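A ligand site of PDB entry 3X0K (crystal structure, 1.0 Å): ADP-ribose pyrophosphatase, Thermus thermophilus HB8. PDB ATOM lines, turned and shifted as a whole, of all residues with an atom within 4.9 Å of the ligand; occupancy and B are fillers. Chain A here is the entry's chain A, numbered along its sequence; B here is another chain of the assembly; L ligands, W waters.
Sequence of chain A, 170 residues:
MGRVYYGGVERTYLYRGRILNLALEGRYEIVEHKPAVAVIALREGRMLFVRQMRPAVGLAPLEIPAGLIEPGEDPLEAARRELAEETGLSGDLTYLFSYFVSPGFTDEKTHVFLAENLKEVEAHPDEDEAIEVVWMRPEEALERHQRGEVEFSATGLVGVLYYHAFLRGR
NH1 of Arg 54 is in salt-bridge range of O6 of the ligand (2.9 Å).
The backbone carbonyl oxygen of Ser 102 of chain B sits close to an oxygen (O7) of the ligand, 3.5 Å away.
O of Glu 29 of chain B is in hydrogen-bond range of N3 of the ligand (2.8 Å).
The backbone NH (N) of Leu 68 sits at hydrogen-bond distance from an oxygen (O5) of the ligand, at 2.8 Å.
A nitrogen (N1) of the ligand sits at hydrogen-bond distance from the backbone NH of Glu 29 of chain B (2.9 Å).
OE2 of Glu 108 sits at hydrogen-bond distance from O10 of the ligand (2.5 Å).
An oxygen (O7) of the ligand is in hydrogen-bond range of the side-chain hydroxyl (OG) of Ser 102 of chain B.
O7 of the ligand lies within hydrogen-bond range of N of Gly 104 of chain B, 2.9 Å away.
The backbone carbonyl oxygen (O) of Gly 104 of chain B lies within hydrogen-bond range of a nitrogen (N3) of the ligand.
OE2 of Glu 108 lies close to ND1 of His 33 (3.5 Å).
The side-chain carboxylate of Glu 63 lies within salt-bridge range of the guanidinium group of Arg 54, 2.8 Å away.
The backbone NH (N) of Ala 66 sits at hydrogen-bond distance from the side-chain carboxylate (OE1) of Glu 86, 3.3 Å away.
The side-chain carboxylate of Glu 108 sits at hydrogen-bond distance from the side-chain hydroxyl of Ser 102 of chain B.
N of Ile 19 lies within hydrogen-bond range of OE1 of Glu 29 of chain B, 2.8 Å away.
The backbone NH (N) of Arg 18 sits at hydrogen-bond distance from the side-chain carboxylate (OE2) of Glu 29 of chain B (2.8 Å).
NH2 of Arg 54 sits close to NE2 of Gln 52 (3.4 Å).
The backbone carbonyl oxygen (O) of Ala 66 sits close to an oxygen (O2) of the ligand (3.4 Å).
NH1 of Arg 18 touches O4 of the ligand, at 3.7 Å.
Ile 19 touches the ligand (CG2 to O11, 3.6 Å).
Ala 36 touches the ligand (CB to O10, 3.9 Å).
OE1 of Glu 63 touches O12 of the ligand (3.9 Å).
Gly 67 touches the ligand (CA to O5, 3.4 Å).
Glu 70 touches the ligand.
Arg 27 of chain B touches the ligand.
Tyr 28 of chain B touches the ligand.
CD of Pro 103 of chain B touches O3 of the ligand, 3.4 Å away.
N of Phe 105 of chain B touches O7 of the ligand (3.8 Å).
Hydrophobic or aromatic side chains that line the ligand: Ile 19, Ala 36, Ala 66, Leu 68, Tyr 28 of chain B and Pro 103 of chain B.
Within 4 Å of the ligand: Arg 18, Ile 19, Ala 36, Arg 54, Glu 63, Ala 66, Gly 67, Leu 68, Glu 70, Glu 108, Arg 27 of chain B, Tyr 28 of chain B, Glu 29 of chain B, Ser 102 of chain B, Pro 103 of chain B, Gly 104 of chain B and Phe 105 of chain B.
Along chain A the residues within 4 Å of the ligand span positions 18 to 108.
The nearest printed residue that does not touch the ligand is Ile 30 of chain B (4.1 Å).
Water W12 bridges an oxygen (O10) of the ligand (2.7 Å) and the side-chain hydroxyl of Thr 110 (2.8 Å).
Water W11 lies within hydrogen-bond range of an oxygen (O5) of the ligand and the side-chain carboxylate of Glu 70.
Water W2 bridges O6 of the ligand (2.7 Å) and O of Gly 104 of chain B (3.2 Å).
Water W8 bridges a ring nitrogen (NE2) of His 33 (2.7 Å) and an oxygen (O7) of the ligand (2.8 Å).
Water W5 lies within hydrogen-bond range of an oxygen (O1) of the ligand, the side-chain amide oxygen of Gln 52 and the side-chain carboxylate of Glu 86.
Water W10 lies within hydrogen-bond range of the guanidinium group (NH1) of Arg 54, a nitrogen (N4) of the ligand and the backbone carbonyl oxygen (O) of Gly 104 of chain B.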
ATOM      1  N   ARG A  18       1.485 -16.296 -23.218  1.00  0.00           N
ATOM      2  CA  ARG A  18       0.493 -17.186 -22.618  1.00  0.00           C
ATOM      3  C   ARG A  18       1.112 -18.379 -21.912  1.00  0.00           C
ATOM      4  O   ARG A  18       0.700 -18.720 -20.782  1.00  0.00           O
ATOM      5  CB  ARG A  18      -0.487 -17.592 -23.717  1.00  0.00           C
ATOM      6  CG  ARG A  18      -1.496 -18.631 -23.233  1.00  0.00           C
ATOM      7  CD  ARG A  18      -2.689 -18.452 -24.154  1.00  0.00           C
ATOM      8  NE  ARG A  18      -3.550 -19.616 -24.170  1.00  0.00           N
ATOM      9  CZ  ARG A  18      -4.684 -19.609 -23.449  1.00  0.00           C
ATOM     10  NH1 ARG A  18      -5.487 -20.664 -23.464  1.00  0.00           N
ATOM     11  NH2 ARG A  18      -4.976 -18.526 -22.742  1.00  0.00           N
ATOM     12  N   ILE A  19       2.024 -18.996 -22.644  1.00  0.00           N
ATOM     13  CA  ILE A  19       2.639 -20.127 -21.852  1.00  0.00           C
ATOM     14  C   ILE A  19       4.142 -19.965 -21.848  1.00  0.00           C
ATOM     15  O   ILE A  19       4.848 -20.933 -21.621  1.00  0.00           O
ATOM     16  CB  ILE A  19       2.307 -21.494 -22.389  1.00  0.00           C
ATOM     17  CG1 ILE A  19       2.926 -21.548 -23.807  1.00  0.00           C
ATOM     18  CG2 ILE A  19       0.860 -21.872 -22.374  1.00  0.00           C
ATOM     19  CD1 ILE A  19       3.344 -23.050 -23.817  1.00  0.00           C
ATOM     20  N   HIS A  33       8.886 -20.706 -18.474  1.00  0.00           N
ATOM     21  CA  HIS A  33       7.750 -21.522 -18.825  1.00  0.00           C
ATOM     22  C   HIS A  33       7.171 -22.128 -17.570  1.00  0.00           C
ATOM     23  O   HIS A  33       7.909 -22.466 -16.666  1.00  0.00           O
ATOM     24  CB  HIS A  33       8.260 -22.641 -19.760  1.00  0.00           C
ATOM     25  CG  HIS A  33       7.231 -23.520 -20.409  1.00  0.00           C
ATOM     26  ND1 HIS A  33       6.459 -24.438 -19.675  1.00  0.00           N
ATOM     27  CD2 HIS A  33       6.902 -23.689 -21.690  1.00  0.00           C
ATOM     28  CE1 HIS A  33       5.714 -25.129 -20.505  1.00  0.00           C
ATOM     29  NE2 HIS A  33       5.936 -24.671 -21.781  1.00  0.00           N
ATOM     30  N   ALA A  36       5.514 -28.392 -15.502  1.00  0.00           N
ATOM     31  CA  ALA A  36       4.655 -29.406 -16.070  1.00  0.00           C
ATOM     32  C   ALA A  36       4.652 -30.648 -15.181  1.00  0.00           C
ATOM     33  O   ALA A  36       5.512 -30.841 -14.314  1.00  0.00           O
ATOM     34  CB  ALA A  36       5.132 -29.787 -17.481  1.00  0.00           C
ATOM     35  N   GLN A  52      -1.366 -35.925 -29.763  1.00  0.00           N
ATOM     36  CA  GLN A  52      -2.132 -34.766 -30.170  1.00  0.00           C
ATOM     37  C   GLN A  52      -1.268 -34.035 -31.209  1.00  0.00           C
ATOM     38  O   GLN A  52      -0.040 -34.085 -31.133  1.00  0.00           O
ATOM     39  CB  GLN A  52      -2.472 -33.823 -29.019  1.00  0.00           C
ATOM     40  CG  GLN A  52      -1.164 -33.273 -28.380  1.00  0.00           C
ATOM     41  CD  GLN A  52      -1.538 -32.754 -27.026  1.00  0.00           C
ATOM     42  OE1 GLN A  52      -2.042 -31.670 -26.860  1.00  0.00           O
ATOM     43  NE2 GLN A  52      -1.282 -33.598 -26.042  1.00  0.00           N
ATOM     44  N   ARG A  54       0.942 -31.351 -32.422  1.00  0.00           N
ATOM     45  CA  ARG A  54       1.788 -30.359 -31.725  1.00  0.00           C
ATOM     46  C   ARG A  54       2.335 -29.429 -32.791  1.00  0.00           C
ATOM     47  O   ARG A  54       3.285 -29.760 -33.492  1.00  0.00           O
ATOM     48  CB  ARG A  54       2.951 -31.127 -31.039  1.00  0.00           C
ATOM     49  CG  ARG A  54       2.464 -31.927 -29.834  1.00  0.00           C
ATOM     50  CD  ARG A  54       1.938 -31.049 -28.717  1.00  0.00           C
ATOM     51  NE  ARG A  54       1.918 -31.764 -27.440  1.00  0.00           N
ATOM     52  CZ  ARG A  54       1.491 -31.208 -26.310  1.00  0.00           C
ATOM     53  NH1 ARG A  54       0.994 -29.977 -26.285  1.00  0.00           N
ATOM     54  NH2 ARG A  54       1.594 -31.909 -25.171  1.00  0.00           N
ATOM     55  N   GLU A  63       3.461 -39.337 -26.366  1.00  0.00           N
ATOM     56  CA  GLU A  63       3.659 -38.740 -25.081  1.00  0.00           C
ATOM     57  C   GLU A  63       2.971 -39.589 -24.029  1.00  0.00           C
ATOM     58  O   GLU A  63       2.208 -40.492 -24.362  1.00  0.00           O
ATOM     59  CB  GLU A  63       3.050 -37.318 -25.037  1.00  0.00           C
ATOM     60  CG  GLU A  63       3.452 -36.479 -26.228  1.00  0.00           C
ATOM     61  CD  GLU A  63       3.042 -35.014 -26.145  1.00  0.00           C
ATOM     62  OE1 GLU A  63       2.896 -34.457 -25.023  1.00  0.00           O
ATOM     63  OE2 GLU A  63       2.880 -34.397 -27.217  1.00  0.00           O
ATOM     64  N   ALA A  66       0.192 -35.467 -19.820  1.00  0.00           N
ATOM     65  CA  ALA A  66       1.085 -34.408 -19.296  1.00  0.00           C
ATOM     66  C   ALA A  66       0.274 -33.100 -19.348  1.00  0.00           C
ATOM     67  O   ALA A  66      -0.629 -32.961 -20.184  1.00  0.00           O
ATOM     68  CB  ALA A  66       2.338 -34.273 -20.126  1.00  0.00           C
ATOM     69  N   GLY A  67       0.659 -32.175 -18.534  1.00  0.00           N
ATOM     70  CA  GLY A  67      -0.044 -30.907 -18.540  1.00  0.00           C
ATOM     71  C   GLY A  67       0.769 -29.869 -17.748  1.00  0.00           C
ATOM     72  O   GLY A  67       1.748 -30.195 -17.093  1.00  0.00           O
ATOM     73  N   LEU A  68       0.299 -28.633 -17.817  1.00  0.00           N
ATOM     74  CA  LEU A  68       0.937 -27.557 -17.047  1.00  0.00           C
ATOM     75  C   LEU A  68       0.321 -27.462 -15.671  1.00  0.00           C
ATOM     76  O   LEU A  68      -0.836 -27.753 -15.448  1.00  0.00           O
ATOM     77  CB  LEU A  68       0.803 -26.221 -17.782  1.00  0.00           C
ATOM     78  CG  LEU A  68       1.385 -26.297 -19.213  1.00  0.00           C
ATOM     79  CD1 LEU A  68       1.320 -24.915 -19.849  1.00  0.00           C
ATOM     80  CD2 LEU A  68       2.792 -26.868 -19.206  1.00  0.00           C
ATOM     81  N   GLU A  70      -1.138 -25.222 -13.084  1.00  0.00           N
ATOM     82  CA  GLU A  70      -1.728 -23.895 -13.114  1.00  0.00           C
ATOM     83  C   GLU A  70      -1.834 -23.254 -11.759  1.00  0.00           C
ATOM     84  O   GLU A  70      -1.544 -23.865 -10.735  1.00  0.00           O
ATOM     85  CB  GLU A  70      -3.089 -24.165 -13.737  1.00  0.00           C
ATOM     86  CG  GLU A  70      -2.934 -24.646 -15.182  1.00  0.00           C
ATOM     87  CD  GLU A  70      -2.485 -23.629 -16.181  1.00  0.00           C
ATOM     88  OE1 GLU A  70      -2.296 -24.142 -17.338  1.00  0.00           O
ATOM     89  OE2 GLU A  70      -2.352 -22.443 -15.888  1.00  0.00           O
ATOM     90  N   GLU A  86      -7.512 -35.655 -19.777  1.00  0.00           N
ATOM     91  CA  GLU A  86      -7.010 -36.203 -21.033  1.00  0.00           C
ATOM     92  C   GLU A  86      -7.487 -37.622 -21.285  1.00  0.00           C
ATOM     93  O   GLU A  86      -7.603 -38.030 -22.460  1.00  0.00           O
ATOM     94  CB  GLU A  86      -5.460 -36.189 -21.035  1.00  0.00           C
ATOM     95  CG  GLU A  86      -4.934 -34.770 -21.115  1.00  0.00           C
ATOM     96  CD  GLU A  86      -3.494 -34.631 -21.524  1.00  0.00           C
ATOM     97  OE1 GLU A  86      -2.648 -35.546 -21.416  1.00  0.00           O
ATOM     98  OE2 GLU A  86      -3.198 -33.534 -22.012  1.00  0.00           O
ATOM     99  N   GLU A 108      11.642 -24.760 -17.836  1.00  0.00           N
ATOM    100  CA  GLU A 108      10.532 -25.719 -17.656  1.00  0.00           C
ATOM    101  C   GLU A 108      11.025 -26.936 -16.906  1.00  0.00           C
ATOM    102  O   GLU A 108      11.983 -27.597 -17.344  1.00  0.00           O
ATOM    103  CB  GLU A 108       9.929 -26.143 -18.989  1.00  0.00           C
ATOM    104  CG  GLU A 108       8.697 -27.005 -18.789  1.00  0.00           C
ATOM    105  CD  GLU A 108       8.097 -27.523 -20.071  1.00  0.00           C
ATOM    106  OE1 GLU A 108       8.748 -27.553 -21.095  1.00  0.00           O
ATOM    107  OE2 GLU A 108       6.874 -27.896 -19.976  1.00  0.00           O
ATOM    108  N   THR A 110       9.585 -30.634 -15.243  1.00  0.00           N
ATOM    109  CA  THR A 110       8.522 -31.637 -15.292  1.00  0.00           C
ATOM    110  C   THR A 110       8.602 -32.542 -14.085  1.00  0.00           C
ATOM    111  O   THR A 110       9.665 -33.101 -13.807  1.00  0.00           O
ATOM    112  CB  THR A 110       8.621 -32.451 -16.573  1.00  0.00           C
ATOM    113  OG1 THR A 110       8.592 -31.527 -17.707  1.00  0.00           O
ATOM    114  CG2 THR A 110       7.479 -33.414 -16.741  1.00  0.00           C
ATOM    115  N   ARG B  27      -2.511 -19.188 -32.677  1.00  0.00           N
ATOM    116  CA  ARG B  27      -2.564 -18.891 -31.240  1.00  0.00           C
ATOM    117  C   ARG B  27      -1.382 -19.456 -30.488  1.00  0.00           C
ATOM    118  O   ARG B  27      -1.124 -19.299 -29.276  1.00  0.00           O
ATOM    119  CB  ARG B  27      -3.895 -19.531 -30.849  1.00  0.00           C
ATOM    120  N   TYR B  28      -0.510 -20.140 -31.171  1.00  0.00           N
ATOM    121  CA  TYR B  28       0.569 -20.908 -30.572  1.00  0.00           C
ATOM    122  C   TYR B  28       1.847 -20.121 -30.556  1.00  0.00           C
ATOM    123  O   TYR B  28       2.283 -19.597 -31.574  1.00  0.00           O
ATOM    124  CB  TYR B  28       0.779 -22.245 -31.332  1.00  0.00           C
ATOM    125  CG  TYR B  28      -0.393 -23.186 -31.123  1.00  0.00           C
ATOM    126  CD1 TYR B  28      -0.357 -24.127 -30.138  1.00  0.00           C
ATOM    127  CD2 TYR B  28      -1.462 -23.099 -31.991  1.00  0.00           C
ATOM    128  CE1 TYR B  28      -1.435 -25.013 -29.943  1.00  0.00           C
ATOM    129  CE2 TYR B  28      -2.535 -23.943 -31.797  1.00  0.00           C
ATOM    130  CZ  TYR B  28      -2.528 -24.891 -30.791  1.00  0.00           C
ATOM    131  OH  TYR B  28      -3.612 -25.737 -30.638  1.00  0.00           O
ATOM    132  N   GLU B  29       2.515 -20.138 -29.430  1.00  0.00           N
ATOM    133  CA  GLU B  29       3.878 -19.590 -29.238  1.00  0.00           C
ATOM    134  C   GLU B  29       4.843 -20.737 -29.406  1.00  0.00           C
ATOM    135  O   GLU B  29       4.745 -21.759 -28.749  1.00  0.00           O
ATOM    136  CB  GLU B  29       3.998 -19.051 -27.827  1.00  0.00           C
ATOM    137  CG  GLU B  29       3.028 -17.858 -27.638  1.00  0.00           C
ATOM    138  CD  GLU B  29       2.703 -17.547 -26.169  1.00  0.00           C
ATOM    139  OE1 GLU B  29       2.920 -18.417 -25.220  1.00  0.00           O
ATOM    140  OE2 GLU B  29       2.229 -16.431 -25.905  1.00  0.00           O
ATOM    141  N   ILE B  30       5.793 -20.537 -30.345  1.00  0.00           N
ATOM    142  CA  ILE B  30       6.695 -21.575 -30.783  1.00  0.00           C
ATOM    143  C   ILE B  30       8.126 -21.114 -30.676  1.00  0.00           C
ATOM    144  O   ILE B  30       8.476 -20.055 -31.197  1.00  0.00           O
ATOM    145  CB  ILE B  30       6.422 -21.941 -32.257  1.00  0.00           C
ATOM    146  CG1 ILE B  30       4.960 -22.346 -32.483  1.00  0.00           C
ATOM    147  CG2 ILE B  30       7.410 -23.028 -32.711  1.00  0.00           C
ATOM    148  CD1 ILE B  30       4.531 -23.338 -31.408  1.00  0.00           C
ATOM    149  N   VAL B 101      12.152 -32.463 -26.716  1.00  0.00           N
ATOM    150  CA  VAL B 101      12.302 -32.098 -25.296  1.00  0.00           C
ATOM    151  C   VAL B 101      10.996 -31.600 -24.678  1.00  0.00           C
ATOM    152  O   VAL B 101      10.776 -31.842 -23.486  1.00  0.00           O
ATOM    153  CB  VAL B 101      13.407 -31.043 -25.012  1.00  0.00           C
ATOM    154  CG1 VAL B 101      14.711 -31.464 -25.694  1.00  0.00           C
ATOM    155  CG2 VAL B 101      13.005 -29.664 -25.525  1.00  0.00           C
ATOM    156  N   SER B 102      10.179 -30.893 -25.472  1.00  0.00           N
ATOM    157  CA  SER B 102       8.939 -30.283 -24.905  1.00  0.00           C
ATOM    158  C   SER B 102       8.106 -29.819 -26.083  1.00  0.00           C
ATOM    159  O   SER B 102       8.077 -28.648 -26.420  1.00  0.00           O
ATOM    160  CB  SER B 102       9.255 -29.159 -23.960  1.00  0.00           C
ATOM    161  OG  SER B 102       8.093 -28.829 -23.267  1.00  0.00           O
ATOM    162  N   PRO B 103       7.455 -30.756 -26.790  1.00  0.00           N
ATOM    163  CA  PRO B 103       6.877 -30.449 -28.101  1.00  0.00           C
ATOM    164  C   PRO B 103       5.629 -29.579 -28.029  1.00  0.00           C
ATOM    165  O   PRO B 103       5.124 -29.203 -29.073  1.00  0.00           O
ATOM    166  CB  PRO B 103       6.592 -31.814 -28.713  1.00  0.00           C
ATOM    167  CG  PRO B 103       6.360 -32.716 -27.486  1.00  0.00           C
ATOM    168  CD  PRO B 103       7.386 -32.220 -26.482  1.00  0.00           C
ATOM    169  N   GLY B 104       5.122 -29.259 -26.814  1.00  0.00           N
ATOM    170  CA  GLY B 104       4.072 -28.268 -26.727  1.00  0.00           C
ATOM    171  C   GLY B 104       4.521 -26.861 -27.011  1.00  0.00           C
ATOM    172  O   GLY B 104       3.649 -26.019 -27.216  1.00  0.00           O
ATOM    173  N   PHE B 105       5.827 -26.573 -27.017  1.00  0.00           N
ATOM    174  CA  PHE B 105       6.242 -25.232 -27.344  1.00  0.00           C
ATOM    175  C   PHE B 105       7.551 -25.136 -28.155  1.00  0.00           C
ATOM    176  O   PHE B 105       7.757 -24.061 -28.725  1.00  0.00           O
ATOM    177  CB  PHE B 105       6.351 -24.313 -26.104  1.00  0.00           C
ATOM    178  CG  PHE B 105       7.677 -24.400 -25.385  1.00  0.00           C
ATOM    179  CD1 PHE B 105       8.655 -23.432 -25.576  1.00  0.00           C
ATOM    180  CD2 PHE B 105       7.942 -25.437 -24.498  1.00  0.00           C
ATOM    181  CE1 PHE B 105       9.871 -23.475 -24.964  1.00  0.00           C
ATOM    182  CE2 PHE B 105       9.199 -25.471 -23.855  1.00  0.00           C
ATOM    183  CZ  PHE B 105      10.132 -24.475 -24.057  1.00  0.00           C
HETATM  184  N1  LIG L   1       1.257 -21.607 -27.230  1.00  0.00           N
HETATM  185  C1  LIG L   1       0.120 -21.120 -26.708  1.00  0.00           C
HETATM  186  N2  LIG L   1      -0.678 -21.767 -25.818  1.00  0.00           N
HETATM  187  C2  LIG L   1      -0.459 -23.104 -25.787  1.00  0.00           C
HETATM  188  C3  LIG L   1       0.608 -23.744 -26.484  1.00  0.00           C
HETATM  189  C4  LIG L   1       1.595 -22.909 -27.116  1.00  0.00           C
HETATM  190  N3  LIG L   1       2.650 -23.445 -27.819  1.00  0.00           N
HETATM  191  N4  LIG L   1       0.534 -25.125 -26.311  1.00  0.00           N
HETATM  192  C5  LIG L   1      -0.519 -25.256 -25.493  1.00  0.00           C
HETATM  193  N5  LIG L   1      -1.169 -24.095 -25.239  1.00  0.00           N
HETATM  194  P1  LIG L   1      -1.789 -28.246 -21.049  1.00  0.00           P
HETATM  195  P2  LIG L   1       0.360 -29.453 -22.652  1.00  0.00           P
HETATM  196  C6  LIG L   1      -2.256 -23.888 -24.250  1.00  0.00           C
HETATM  197  O1  LIG L   1      -2.720 -28.823 -21.924  1.00  0.00           O
HETATM  198  O2  LIG L   1      -0.189 -30.830 -22.808  1.00  0.00           O
HETATM  199  C7  LIG L   1       4.714 -31.115 -23.543  1.00  0.00           C
HETATM  200  O3  LIG L   1       6.028 -31.625 -23.403  1.00  0.00           O
HETATM  201  C8  LIG L   1      -3.406 -24.817 -24.522  1.00  0.00           C
HETATM  202  O4  LIG L   1      -4.605 -24.088 -24.660  1.00  0.00           O
HETATM  203  O5  LIG L   1      -1.920 -28.297 -19.573  1.00  0.00           O
HETATM  204  O6  LIG L   1       0.280 -28.536 -23.825  1.00  0.00           O
HETATM  205  C9  LIG L   1       4.621 -29.655 -23.338  1.00  0.00           C
HETATM  206  O7  LIG L   1       5.614 -28.866 -23.951  1.00  0.00           O
HETATM  207  C10 LIG L   1      -3.588 -25.607 -23.221  1.00  0.00           C
HETATM  208  O8  LIG L   1      -4.930 -25.937 -22.965  1.00  0.00           O
HETATM  209  O9  LIG L   1      -0.327 -28.777 -21.365  1.00  0.00           O
HETATM  210  C11 LIG L   1       4.622 -29.538 -21.811  1.00  0.00           C
HETATM  211  O10 LIG L   1       5.963 -29.741 -21.336  1.00  0.00           O
HETATM  212  C12 LIG L   1      -2.901 -24.792 -22.195  1.00  0.00           C
HETATM  213  O11 LIG L   1      -1.866 -24.131 -22.901  1.00  0.00           O
HETATM  214  C13 LIG L   1       3.756 -30.699 -21.404  1.00  0.00           C
HETATM  215  O12 LIG L   1       3.868 -31.648 -22.501  1.00  0.00           O
HETATM  216  C14 LIG L   1      -2.460 -25.598 -20.978  1.00  0.00           C
HETATM  217  O13 LIG L   1      -1.638 -26.626 -21.368  1.00  0.00           O
HETATM  218  C15 LIG L   1       2.318 -30.386 -21.160  1.00  0.00           C
HETATM  219  O14 LIG L   1       1.849 -29.463 -22.184  1.00  0.00           O
HETATM  220  O   HOH W   1      -3.506 -29.697 -18.127  1.00  0.00           O
HETATM  221  O   HOH W   2       2.266 -26.762 -24.431  1.00  0.00           O
HETATM  222  O   HOH W   3      -5.514 -28.387 -21.164  1.00  0.00           O
HETATM  223  O   HOH W   4       4.715 -34.384 -22.994  1.00  0.00           O
HETATM  224  O   HOH W   5      -3.018 -30.972 -24.039  1.00  0.00           O
HETATM  225  O   HOH W   6      -6.478 -25.076 -21.191  1.00  0.00           O
HETATM  226  O   HOH W   7      -1.963 -28.202 -25.406  1.00  0.00           O
HETATM  227  O   HOH W   8       4.711 -26.284 -23.531  1.00  0.00           O
HETATM  228  O   HOH W   9      -0.974 -33.366 -23.193  1.00  0.00           O
HETATM  229  O   HOH W  10       1.028 -27.630 -28.301  1.00  0.00           O
HETATM  230  O   HOH W  11      -3.364 -26.852 -17.775  1.00  0.00           O
HETATM  231  O   HOH W  12       7.207 -31.796 -20.105  1.00  0.00           O
HETATM  232  O   HOH W  13       7.632 -34.288 -23.372  1.00  0.00           O
